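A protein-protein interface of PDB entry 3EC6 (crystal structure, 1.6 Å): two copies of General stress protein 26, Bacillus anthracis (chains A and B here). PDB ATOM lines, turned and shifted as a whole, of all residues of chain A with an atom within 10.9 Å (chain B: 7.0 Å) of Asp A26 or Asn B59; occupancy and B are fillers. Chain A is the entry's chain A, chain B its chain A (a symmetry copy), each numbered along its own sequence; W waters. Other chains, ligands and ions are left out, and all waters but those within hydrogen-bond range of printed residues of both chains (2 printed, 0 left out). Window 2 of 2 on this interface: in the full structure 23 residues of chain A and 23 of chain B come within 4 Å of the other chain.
The backbone carbonyl oxygen of Asp A26 lies within hydrogen-bond range of the side-chain amide nitrogen of Asn B59, 3.1 Å away.
The side-chain amide nitrogen (ND2) of Asn A59 is in hydrogen-bond range of the backbone carbonyl oxygen (O) of Asp B26 (3.1 Å).
OD1 of Asn A61 lies close to OD1 of Asn A59, at 2.9 Å.
The side-chain amino group (NZ) of Lys B52 is in hydrogen-bond range of the side-chain hydroxyl (OG1) of Thr B22.
The side-chain hydroxyl (OG1) of Thr B22 sits at hydrogen-bond distance from the side-chain carboxylate (OD2) of Asp B55.
The side-chain amide oxygen of Asn B59 sits close to the side-chain amide oxygen of Asn B61, at 2.9 Å.
Val B23 touches Lys A27.
Lys A27 touches Asn B61.
Pro A28 touches Thr B22 (CB to O, 3.6 Å).
Val B23 touches Pro A28.
O of Asn B61 touches CD of Pro A28, 3.3 Å away.
Pro A28 touches Val B62.
Of the printed residues of chain B, Asp A26 touches Asn B59.
No residue of chain A comes within 4 Å of Pro B60.
Asn B61 touches two residues of chain A.
Of the printed residues of chain A, Val B23 touches Lys A27 (3.98 Å) and Pro A28 (3.7 Å).
Printed residues of chain A within 4 Å of Thr B22: Pro A28.
Of the printed residues of chain A, Val B62 touches Pro A28.
Of the printed residues of chain B, Asn A59 touches Asp B26.
The nearest residue of chain A that does not touch Asn B59 is Lys A27 (5.1 Å).
The nearest printed residue of chain B that does not touch Asn A59 is Val B23 (6.8 Å).
Along chain A the printed residues that touch a printed residue of chain B span positions 26 to 59.
Hydrophobic or aromatic side chains of chain B within 4 Å of the printed part of chain A: Val B23.
Asp A26 touches Asn B59, and with the chains exchanged Asn A59 touches Asp B26.
Positions printed for both chains: 22, 23, 24, 26, 54, 55, 56, 58, 59 and 61.
Of the 8 pairs that touch across the chains among the printed residues, 2 have their exchanged pair printed and touching as well.
Water W1 lies within hydrogen-bond range of the side-chain amide nitrogen (ND2) of Asn B59 (2.8 Å) and the side-chain carboxylate (OD1) of Asp A26 (3.0 Å).
Water W2 lies within hydrogen-bond range of ND2 of Asn A59 (2.8 Å) and OD1 of Asp B26 (3.0 Å).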
ATOM      1  N   THR A  22      20.088 -16.486  -6.005  1.00  0.00           N
ATOM      2  CA  THR A  22      20.245 -16.084  -7.396  1.00  0.00           C
ATOM      3  C   THR A  22      21.724 -16.118  -7.727  1.00  0.00           C
ATOM      4  O   THR A  22      22.578 -16.401  -6.849  1.00  0.00           O
ATOM      5  CB  THR A  22      19.762 -14.612  -7.593  1.00  0.00           C
ATOM      6  OG1 THR A  22      20.375 -13.787  -6.566  1.00  0.00           O
ATOM      7  CG2 THR A  22      18.225 -14.515  -7.472  1.00  0.00           C
ATOM      8  N   VAL A  23      22.038 -15.937  -9.023  1.00  0.00           N
ATOM      9  CA  VAL A  23      23.428 -15.769  -9.468  1.00  0.00           C
ATOM     10  C   VAL A  23      23.660 -14.305  -9.803  1.00  0.00           C
ATOM     11  O   VAL A  23      22.834 -13.705 -10.504  1.00  0.00           O
ATOM     12  CB  VAL A  23      23.716 -16.610 -10.713  1.00  0.00           C
ATOM     13  CG1 VAL A  23      25.191 -16.401 -11.167  1.00  0.00           C
ATOM     14  CG2 VAL A  23      23.431 -18.050 -10.445  1.00  0.00           C
ATOM     15  N   ARG A  24      24.752 -13.737  -9.283  1.00  0.00           N
ATOM     16  CA  ARG A  24      25.042 -12.279  -9.307  1.00  0.00           C
ATOM     17  C   ARG A  24      26.463 -12.196  -9.787  1.00  0.00           C
ATOM     18  O   ARG A  24      27.410 -12.468  -9.032  1.00  0.00           O
ATOM     19  CB  ARG A  24      24.925 -11.642  -7.907  1.00  0.00           C
ATOM     20  CG  ARG A  24      25.294 -10.133  -7.862  1.00  0.00           C
ATOM     21  CD  ARG A  24      24.854  -9.421  -6.592  1.00  0.00           C
ATOM     22  NE  ARG A  24      23.438  -9.587  -6.394  1.00  0.00           N
ATOM     23  CZ  ARG A  24      22.762  -9.285  -5.280  1.00  0.00           C
ATOM     24  NH1 ARG A  24      23.365  -8.723  -4.232  1.00  0.00           N
ATOM     25  NH2 ARG A  24      21.463  -9.527  -5.256  1.00  0.00           N
ATOM     26  N   ASN A  25      26.621 -11.856 -11.052  1.00  0.00           N
ATOM     27  CA  ASN A  25      27.965 -11.724 -11.607  1.00  0.00           C
ATOM     28  C   ASN A  25      28.788 -13.005 -11.455  1.00  0.00           C
ATOM     29  O   ASN A  25      29.955 -12.970 -11.014  1.00  0.00           O
ATOM     30  CB  ASN A  25      28.679 -10.567 -10.908  1.00  0.00           C
ATOM     31  CG  ASN A  25      28.116  -9.242 -11.290  1.00  0.00           C
ATOM     32  OD1 ASN A  25      27.768  -9.016 -12.455  1.00  0.00           O
ATOM     33  ND2 ASN A  25      27.994  -8.349 -10.307  1.00  0.00           N
ATOM     34  N   ASP A  26      28.159 -14.145 -11.755  1.00  0.00           N
ATOM     35  CA  ASP A  26      28.851 -15.429 -11.735  1.00  0.00           C
ATOM     36  C   ASP A  26      29.238 -15.866 -10.283  1.00  0.00           C
ATOM     37  O   ASP A  26      30.157 -16.648 -10.056  1.00  0.00           O
ATOM     38  CB  ASP A  26      30.069 -15.304 -12.637  1.00  0.00           C
ATOM     39  CG  ASP A  26      30.520 -16.620 -13.220  1.00  0.00           C
ATOM     40  OD1 ASP A  26      29.763 -17.612 -13.145  1.00  0.00           O
ATOM     41  OD2 ASP A  26      31.652 -16.662 -13.770  1.00  0.00           O
ATOM     42  N   LYS A  27      28.520 -15.334  -9.302  1.00  0.00           N
ATOM     43  CA  LYS A  27      28.697 -15.739  -7.903  1.00  0.00           C
ATOM     44  C   LYS A  27      27.307 -15.924  -7.290  1.00  0.00           C
ATOM     45  O   LYS A  27      26.345 -15.293  -7.744  1.00  0.00           O
ATOM     46  CB  LYS A  27      29.416 -14.640  -7.130  1.00  0.00           C
ATOM     47  CG  LYS A  27      30.779 -14.316  -7.726  1.00  0.00           C
ATOM     48  CD  LYS A  27      31.494 -13.298  -6.868  1.00  0.00           C
ATOM     49  CE  LYS A  27      30.671 -12.095  -6.521  1.00  0.00           C
ATOM     50  NZ  LYS A  27      31.593 -11.057  -5.909  1.00  0.00           N
ATOM     51  N   PRO A  28      27.188 -16.819  -6.304  1.00  0.00           N
ATOM     52  CA  PRO A  28      25.879 -17.019  -5.691  1.00  0.00           C
ATOM     53  C   PRO A  28      25.551 -15.894  -4.693  1.00  0.00           C
ATOM     54  O   PRO A  28      26.433 -15.304  -4.049  1.00  0.00           O
ATOM     55  CB  PRO A  28      26.033 -18.354  -4.939  1.00  0.00           C
ATOM     56  CG  PRO A  28      27.524 -18.322  -4.495  1.00  0.00           C
ATOM     57  CD  PRO A  28      28.285 -17.516  -5.604  1.00  0.00           C
ATOM     58  N   HIS A  29      24.266 -15.600  -4.585  1.00  0.00           N
ATOM     59  CA  HIS A  29      23.777 -14.644  -3.590  1.00  0.00           C
ATOM     60  C   HIS A  29      22.488 -15.171  -3.019  1.00  0.00           C
ATOM     61  O   HIS A  29      21.600 -15.595  -3.769  1.00  0.00           O
ATOM     62  CB  HIS A  29      23.492 -13.297  -4.215  1.00  0.00           C
ATOM     63  CG  HIS A  29      22.983 -12.307  -3.216  1.00  0.00           C
ATOM     64  ND1 HIS A  29      21.638 -12.154  -2.923  1.00  0.00           N
ATOM     65  CD2 HIS A  29      23.651 -11.442  -2.407  1.00  0.00           C
ATOM     66  CE1 HIS A  29      21.502 -11.210  -2.002  1.00  0.00           C
ATOM     67  NE2 HIS A  29      22.712 -10.761  -1.679  1.00  0.00           N
ATOM     68  N   THR A  54      17.924  -7.216 -10.459  1.00  0.00           N
ATOM     69  CA  THR A  54      18.994  -7.179 -11.442  1.00  0.00           C
ATOM     70  C   THR A  54      19.617  -8.555 -11.704  1.00  0.00           C
ATOM     71  O   THR A  54      19.947  -8.869 -12.852  1.00  0.00           O
ATOM     72  CB  THR A  54      20.090  -6.195 -10.982  1.00  0.00           C
ATOM     73  OG1 THR A  54      19.446  -4.934 -10.772  1.00  0.00           O
ATOM     74  CG2 THR A  54      21.199  -6.021 -12.050  1.00  0.00           C
ATOM     75  N   ASP A  55      19.760  -9.345 -10.629  1.00  0.00           N
ATOM     76  CA  ASP A  55      20.309 -10.713 -10.743  1.00  0.00           C
ATOM     77  C   ASP A  55      19.434 -11.462 -11.726  1.00  0.00           C
ATOM     78  O   ASP A  55      19.952 -12.035 -12.704  1.00  0.00           O
ATOM     79  CB  ASP A  55      20.292 -11.495  -9.431  1.00  0.00           C
ATOM     80  CG  ASP A  55      21.235 -10.968  -8.404  1.00  0.00           C
ATOM     81  OD1 ASP A  55      22.159 -10.169  -8.743  1.00  0.00           O
ATOM     82  OD2 ASP A  55      21.063 -11.367  -7.247  1.00  0.00           O
ATOM     83  N   ILE A  56      18.122 -11.442 -11.432  1.00  0.00           N
ATOM     84  CA  ILE A  56      17.124 -12.242 -12.193  1.00  0.00           C
ATOM     85  C   ILE A  56      17.161 -11.742 -13.630  1.00  0.00           C
ATOM     86  O   ILE A  56      17.137 -12.532 -14.547  1.00  0.00           O
ATOM     87  CB  ILE A  56      15.711 -12.270 -11.523  1.00  0.00           C
ATOM     88  CG1 ILE A  56      15.775 -13.091 -10.216  1.00  0.00           C
ATOM     89  CG2 ILE A  56      14.570 -12.800 -12.456  1.00  0.00           C
ATOM     90  CD1 ILE A  56      14.568 -12.954  -9.308  1.00  0.00           C
ATOM     91  N   ASN A  58      19.646 -10.826 -15.210  1.00  0.00           N
ATOM     92  CA  ASN A  58      20.839 -11.403 -15.862  1.00  0.00           C
ATOM     93  C   ASN A  58      20.898 -12.978 -15.990  1.00  0.00           C
ATOM     94  O   ASN A  58      21.487 -13.563 -16.894  1.00  0.00           O
ATOM     95  CB  ASN A  58      22.090 -10.805 -15.178  1.00  0.00           C
ATOM     96  CG  ASN A  58      22.277  -9.305 -15.519  1.00  0.00           C
ATOM     97  OD1 ASN A  58      22.544  -8.948 -16.696  1.00  0.00           O
ATOM     98  ND2 ASN A  58      22.120  -8.430 -14.524  1.00  0.00           N
ATOM     99  N   ASN A  59      20.181 -13.647 -15.111  1.00  0.00           N
ATOM    100  CA  ASN A  59      20.130 -15.086 -15.147  1.00  0.00           C
ATOM    101  C   ASN A  59      18.854 -15.414 -14.418  1.00  0.00           C
ATOM    102  O   ASN A  59      18.722 -15.143 -13.239  1.00  0.00           O
ATOM    103  CB  ASN A  59      21.351 -15.697 -14.393  1.00  0.00           C
ATOM    104  CG  ASN A  59      21.360 -17.215 -14.400  1.00  0.00           C
ATOM    105  OD1 ASN A  59      20.309 -17.873 -14.425  1.00  0.00           O
ATOM    106  ND2 ASN A  59      22.540 -17.802 -14.267  1.00  0.00           N
ATOM    107  N   ASN A  61      17.520 -18.224 -13.419  1.00  0.00           N
ATOM    108  CA  ASN A  61      17.465 -19.453 -12.589  1.00  0.00           C
ATOM    109  C   ASN A  61      17.612 -19.099 -11.131  1.00  0.00           C
ATOM    110  O   ASN A  61      18.541 -18.377 -10.763  1.00  0.00           O
ATOM    111  CB  ASN A  61      18.609 -20.382 -12.957  1.00  0.00           C
ATOM    112  CG  ASN A  61      18.477 -20.910 -14.358  1.00  0.00           C
ATOM    113  OD1 ASN A  61      19.055 -20.345 -15.296  1.00  0.00           O
ATOM    114  ND2 ASN A  61      17.710 -21.943 -14.512  1.00  0.00           N
ATOM    115  N   THR B  22      26.192 -21.907  -3.372  1.00  0.00           N
ATOM    116  CA  THR B  22      27.214 -22.149  -4.383  1.00  0.00           C
ATOM    117  C   THR B  22      26.565 -22.001  -5.745  1.00  0.00           C
ATOM    118  O   THR B  22      25.334 -21.770  -5.855  1.00  0.00           O
ATOM    119  CB  THR B  22      27.742 -23.614  -4.279  1.00  0.00           C
ATOM    120  OG1 THR B  22      26.601 -24.511  -4.229  1.00  0.00           O
ATOM    121  CG2 THR B  22      28.594 -23.805  -3.006  1.00  0.00           C
ATOM    122  N   VAL B  23      27.403 -22.025  -6.798  1.00  0.00           N
ATOM    123  CA  VAL B  23      26.910 -22.071  -8.181  1.00  0.00           C
ATOM    124  C   VAL B  23      27.109 -23.476  -8.724  1.00  0.00           C
ATOM    125  O   VAL B  23      28.199 -24.041  -8.563  1.00  0.00           O
ATOM    126  CB  VAL B  23      27.669 -21.087  -9.073  1.00  0.00           C
ATOM    127  CG1 VAL B  23      27.134 -21.168 -10.532  1.00  0.00           C
ATOM    128  CG2 VAL B  23      27.558 -19.701  -8.530  1.00  0.00           C
ATOM    129  N   ARG B  24      26.059 -24.038  -9.330  1.00  0.00           N
ATOM    130  CA  ARG B  24      25.977 -25.468  -9.730  1.00  0.00           C
ATOM    131  C   ARG B  24      25.488 -25.424 -11.149  1.00  0.00           C
ATOM    132  O   ARG B  24      24.298 -25.185 -11.409  1.00  0.00           O
ATOM    133  CB  ARG B  24      24.980 -26.257  -8.858  1.00  0.00           C
ATOM    134  CG  ARG B  24      24.797 -27.741  -9.283  1.00  0.00           C
ATOM    135  CD  ARG B  24      24.103 -28.607  -8.243  1.00  0.00           C
ATOM    136  NE  ARG B  24      24.807 -28.539  -6.989  1.00  0.00           N
ATOM    137  CZ  ARG B  24      24.360 -28.993  -5.814  1.00  0.00           C
ATOM    138  NH1 ARG B  24      23.194 -29.632  -5.714  1.00  0.00           N
ATOM    139  NH2 ARG B  24      25.125 -28.824  -4.750  1.00  0.00           N
ATOM    140  N   ASP B  26      25.896 -23.189 -13.470  1.00  0.00           N
ATOM    141  CA  ASP B  26      25.388 -21.879 -13.865  1.00  0.00           C
ATOM    142  C   ASP B  26      23.983 -21.581 -13.243  1.00  0.00           C
ATOM    143  O   ASP B  26      23.200 -20.781 -13.746  1.00  0.00           O
ATOM    144  CB  ASP B  26      25.359 -21.843 -15.385  1.00  0.00           C
ATOM    145  CG  ASP B  26      25.472 -20.450 -15.953  1.00  0.00           C
ATOM    146  OD1 ASP B  26      25.824 -19.513 -15.204  1.00  0.00           O
ATOM    147  OD2 ASP B  26      25.209 -20.289 -17.174  1.00  0.00           O
ATOM    148  N   LYS B  52      27.962 -30.145  -3.085  1.00  0.00           N
ATOM    149  CA  LYS B  52      28.536 -28.830  -2.752  1.00  0.00           C
ATOM    150  C   LYS B  52      30.033 -28.851  -2.992  1.00  0.00           C
ATOM    151  O   LYS B  52      30.609 -27.867  -3.406  1.00  0.00           O
ATOM    152  CB  LYS B  52      28.283 -28.453  -1.293  1.00  0.00           C
ATOM    153  CG  LYS B  52      26.829 -28.394  -0.902  1.00  0.00           C
ATOM    154  CD  LYS B  52      26.052 -27.355  -1.734  1.00  0.00           C
ATOM    155  CE  LYS B  52      25.765 -26.114  -1.003  1.00  0.00           C
ATOM    156  NZ  LYS B  52      25.094 -25.133  -1.894  1.00  0.00           N
ATOM    157  N   THR B  54      31.517 -30.746  -5.363  1.00  0.00           N
ATOM    158  CA  THR B  54      31.637 -30.621  -6.806  1.00  0.00           C
ATOM    159  C   THR B  54      31.390 -29.194  -7.308  1.00  0.00           C
ATOM    160  O   THR B  54      32.075 -28.742  -8.231  1.00  0.00           O
ATOM    161  CB  THR B  54      30.655 -31.590  -7.497  1.00  0.00           C
ATOM    162  OG1 THR B  54      30.951 -32.898  -6.997  1.00  0.00           O
ATOM    163  CG2 THR B  54      30.826 -31.589  -9.036  1.00  0.00           C
ATOM    164  N   ASP B  55      30.414 -28.517  -6.684  1.00  0.00           N
ATOM    165  CA  ASP B  55      30.094 -27.118  -7.039  1.00  0.00           C
ATOM    166  C   ASP B  55      31.366 -26.315  -6.865  1.00  0.00           C
ATOM    167  O   ASP B  55      31.789 -25.613  -7.805  1.00  0.00           O
ATOM    168  CB  ASP B  55      29.030 -26.484  -6.146  1.00  0.00           C
ATOM    169  CG  ASP B  55      27.670 -27.067  -6.323  1.00  0.00           C
ATOM    170  OD1 ASP B  55      27.412 -27.776  -7.343  1.00  0.00           O
ATOM    171  OD2 ASP B  55      26.842 -26.804  -5.444  1.00  0.00           O
ATOM    172  N   ILE B  56      31.940 -26.435  -5.656  1.00  0.00           N
ATOM    173  CA  ILE B  56      33.110 -25.613  -5.244  1.00  0.00           C
ATOM    174  C   ILE B  56      34.246 -25.953  -6.198  1.00  0.00           C
ATOM    175  O   ILE B  56      34.942 -25.071  -6.650  1.00  0.00           O
ATOM    176  CB  ILE B  56      33.448 -25.731  -3.722  1.00  0.00           C
ATOM    177  CG1 ILE B  56      32.335 -25.053  -2.891  1.00  0.00           C
ATOM    178  CG2 ILE B  56      34.855 -25.165  -3.331  1.00  0.00           C
ATOM    179  CD1 ILE B  56      32.367 -25.350  -1.404  1.00  0.00           C
ATOM    180  N   GLU B  57      34.427 -27.242  -6.490  1.00  0.00           N
ATOM    181  CA  GLU B  57      35.375 -27.691  -7.535  1.00  0.00           C
ATOM    182  C   GLU B  57      35.239 -26.940  -8.851  1.00  0.00           C
ATOM    183  O   GLU B  57      36.230 -26.713  -9.565  1.00  0.00           O
ATOM    184  CB  GLU B  57      35.242 -29.212  -7.806  1.00  0.00           C
ATOM    185  CG  GLU B  57      35.799 -30.127  -6.731  1.00  0.00           C
ATOM    186  CD  GLU B  57      35.397 -31.602  -6.921  1.00  0.00           C
ATOM    187  OE1 GLU B  57      34.950 -31.982  -8.014  1.00  0.00           O
ATOM    188  OE2 GLU B  57      35.574 -32.387  -5.981  1.00  0.00           O
ATOM    189  N   ASN B  58      34.015 -26.562  -9.212  1.00  0.00           N
ATOM    190  CA  ASN B  58      33.766 -25.855 -10.487  1.00  0.00           C
ATOM    191  C   ASN B  58      33.749 -24.275 -10.441  1.00  0.00           C
ATOM    192  O   ASN B  58      34.068 -23.566 -11.390  1.00  0.00           O
ATOM    193  CB  ASN B  58      32.492 -26.457 -11.121  1.00  0.00           C
ATOM    194  CG  ASN B  58      32.725 -27.899 -11.636  1.00  0.00           C
ATOM    195  OD1 ASN B  58      33.507 -28.114 -12.599  1.00  0.00           O
ATOM    196  ND2 ASN B  58      32.084 -28.884 -11.004  1.00  0.00           N
ATOM    197  N   ASN B  59      33.461 -23.743  -9.271  1.00  0.00           N
ATOM    198  CA  ASN B  59      33.444 -22.314  -9.098  1.00  0.00           C
ATOM    199  C   ASN B  59      33.635 -22.133  -7.615  1.00  0.00           C
ATOM    200  O   ASN B  59      32.801 -22.535  -6.826  1.00  0.00           O
ATOM    201  CB  ASN B  59      32.069 -21.723  -9.538  1.00  0.00           C
ATOM    202  CG  ASN B  59      31.988 -20.214  -9.386  1.00  0.00           C
ATOM    203  OD1 ASN B  59      32.618 -19.614  -8.502  1.00  0.00           O
ATOM    204  ND2 ASN B  59      31.129 -19.584 -10.172  1.00  0.00           N
ATOM    205  N   PRO B  60      34.752 -21.489  -7.202  1.00  0.00           N
ATOM    206  CA  PRO B  60      35.028 -21.458  -5.768  1.00  0.00           C
ATOM    207  C   PRO B  60      34.273 -20.371  -4.962  1.00  0.00           C
ATOM    208  O   PRO B  60      34.410 -20.319  -3.730  1.00  0.00           O
ATOM    209  CB  PRO B  60      36.544 -21.133  -5.709  1.00  0.00           C
ATOM    210  CG  PRO B  60      36.810 -20.307  -6.885  1.00  0.00           C
ATOM    211  CD  PRO B  60      35.835 -20.873  -8.006  1.00  0.00           C
ATOM    212  N   ASN B  61      33.518 -19.521  -5.657  1.00  0.00           N
ATOM    213  CA  ASN B  61      32.833 -18.392  -4.979  1.00  0.00           C
ATOM    214  C   ASN B  61      31.613 -18.893  -4.249  1.00  0.00           C
ATOM    215  O   ASN B  61      30.791 -19.600  -4.835  1.00  0.00           O
ATOM    216  CB  ASN B  61      32.372 -17.370  -6.004  1.00  0.00           C
ATOM    217  CG  ASN B  61      33.529 -16.703  -6.692  1.00  0.00           C
ATOM    218  OD1 ASN B  61      33.944 -17.132  -7.777  1.00  0.00           O
ATOM    219  ND2 ASN B  61      34.067 -15.701  -6.070  1.00  0.00           N
ATOM    220  N   VAL B  62      31.544 -18.558  -2.969  1.00  0.00           N
ATOM    221  CA  VAL B  62      30.394 -19.005  -2.145  1.00  0.00           C
ATOM    222  C   VAL B  62      29.839 -17.850  -1.368  1.00  0.00           C
ATOM    223  O   VAL B  62      30.440 -16.792  -1.252  1.00  0.00           O
ATOM    224  CB  VAL B  62      30.810 -20.126  -1.140  1.00  0.00           C
ATOM    225  CG1 VAL B  62      31.355 -21.331  -1.912  1.00  0.00           C
ATOM    226  CG2 VAL B  62      31.814 -19.624  -0.088  1.00  0.00           C
ATOM    227  N   LEU B  83      35.917 -17.136  -1.187  1.00  0.00           N
ATOM    228  CA  LEU B  83      36.268 -18.352  -1.934  1.00  0.00           C
ATOM    229  C   LEU B  83      36.458 -19.530  -0.996  1.00  0.00           C
ATOM    230  O   LEU B  83      37.008 -19.397   0.096  1.00  0.00           O
ATOM    231  CB  LEU B  83      37.531 -18.124  -2.773  1.00  0.00           C
ATOM    232  CG  LEU B  83      37.350 -17.421  -4.123  1.00  0.00           C
ATOM    233  CD1 LEU B  83      36.891 -15.966  -3.967  1.00  0.00           C
ATOM    234  CD2 LEU B  83      38.640 -17.482  -4.926  1.00  0.00           C
ATOM    235  N   ALA B  84      35.960 -20.682  -1.428  1.00  0.00           N
ATOM    236  CA  ALA B  84      36.024 -21.897  -0.677  1.00  0.00           C
ATOM    237  C   ALA B  84      37.092 -22.839  -1.232  1.00  0.00           C
ATOM    238  O   ALA B  84      37.456 -22.813  -2.426  1.00  0.00           O
ATOM    239  CB  ALA B  84      34.642 -22.567  -0.757  1.00  0.00           C
HETATM  240  O   HOH W   1      30.012 -20.594 -12.560  1.00  0.00           O
HETATM  241  O   HOH W   2      25.054 -16.602 -14.726  1.00  0.00           O
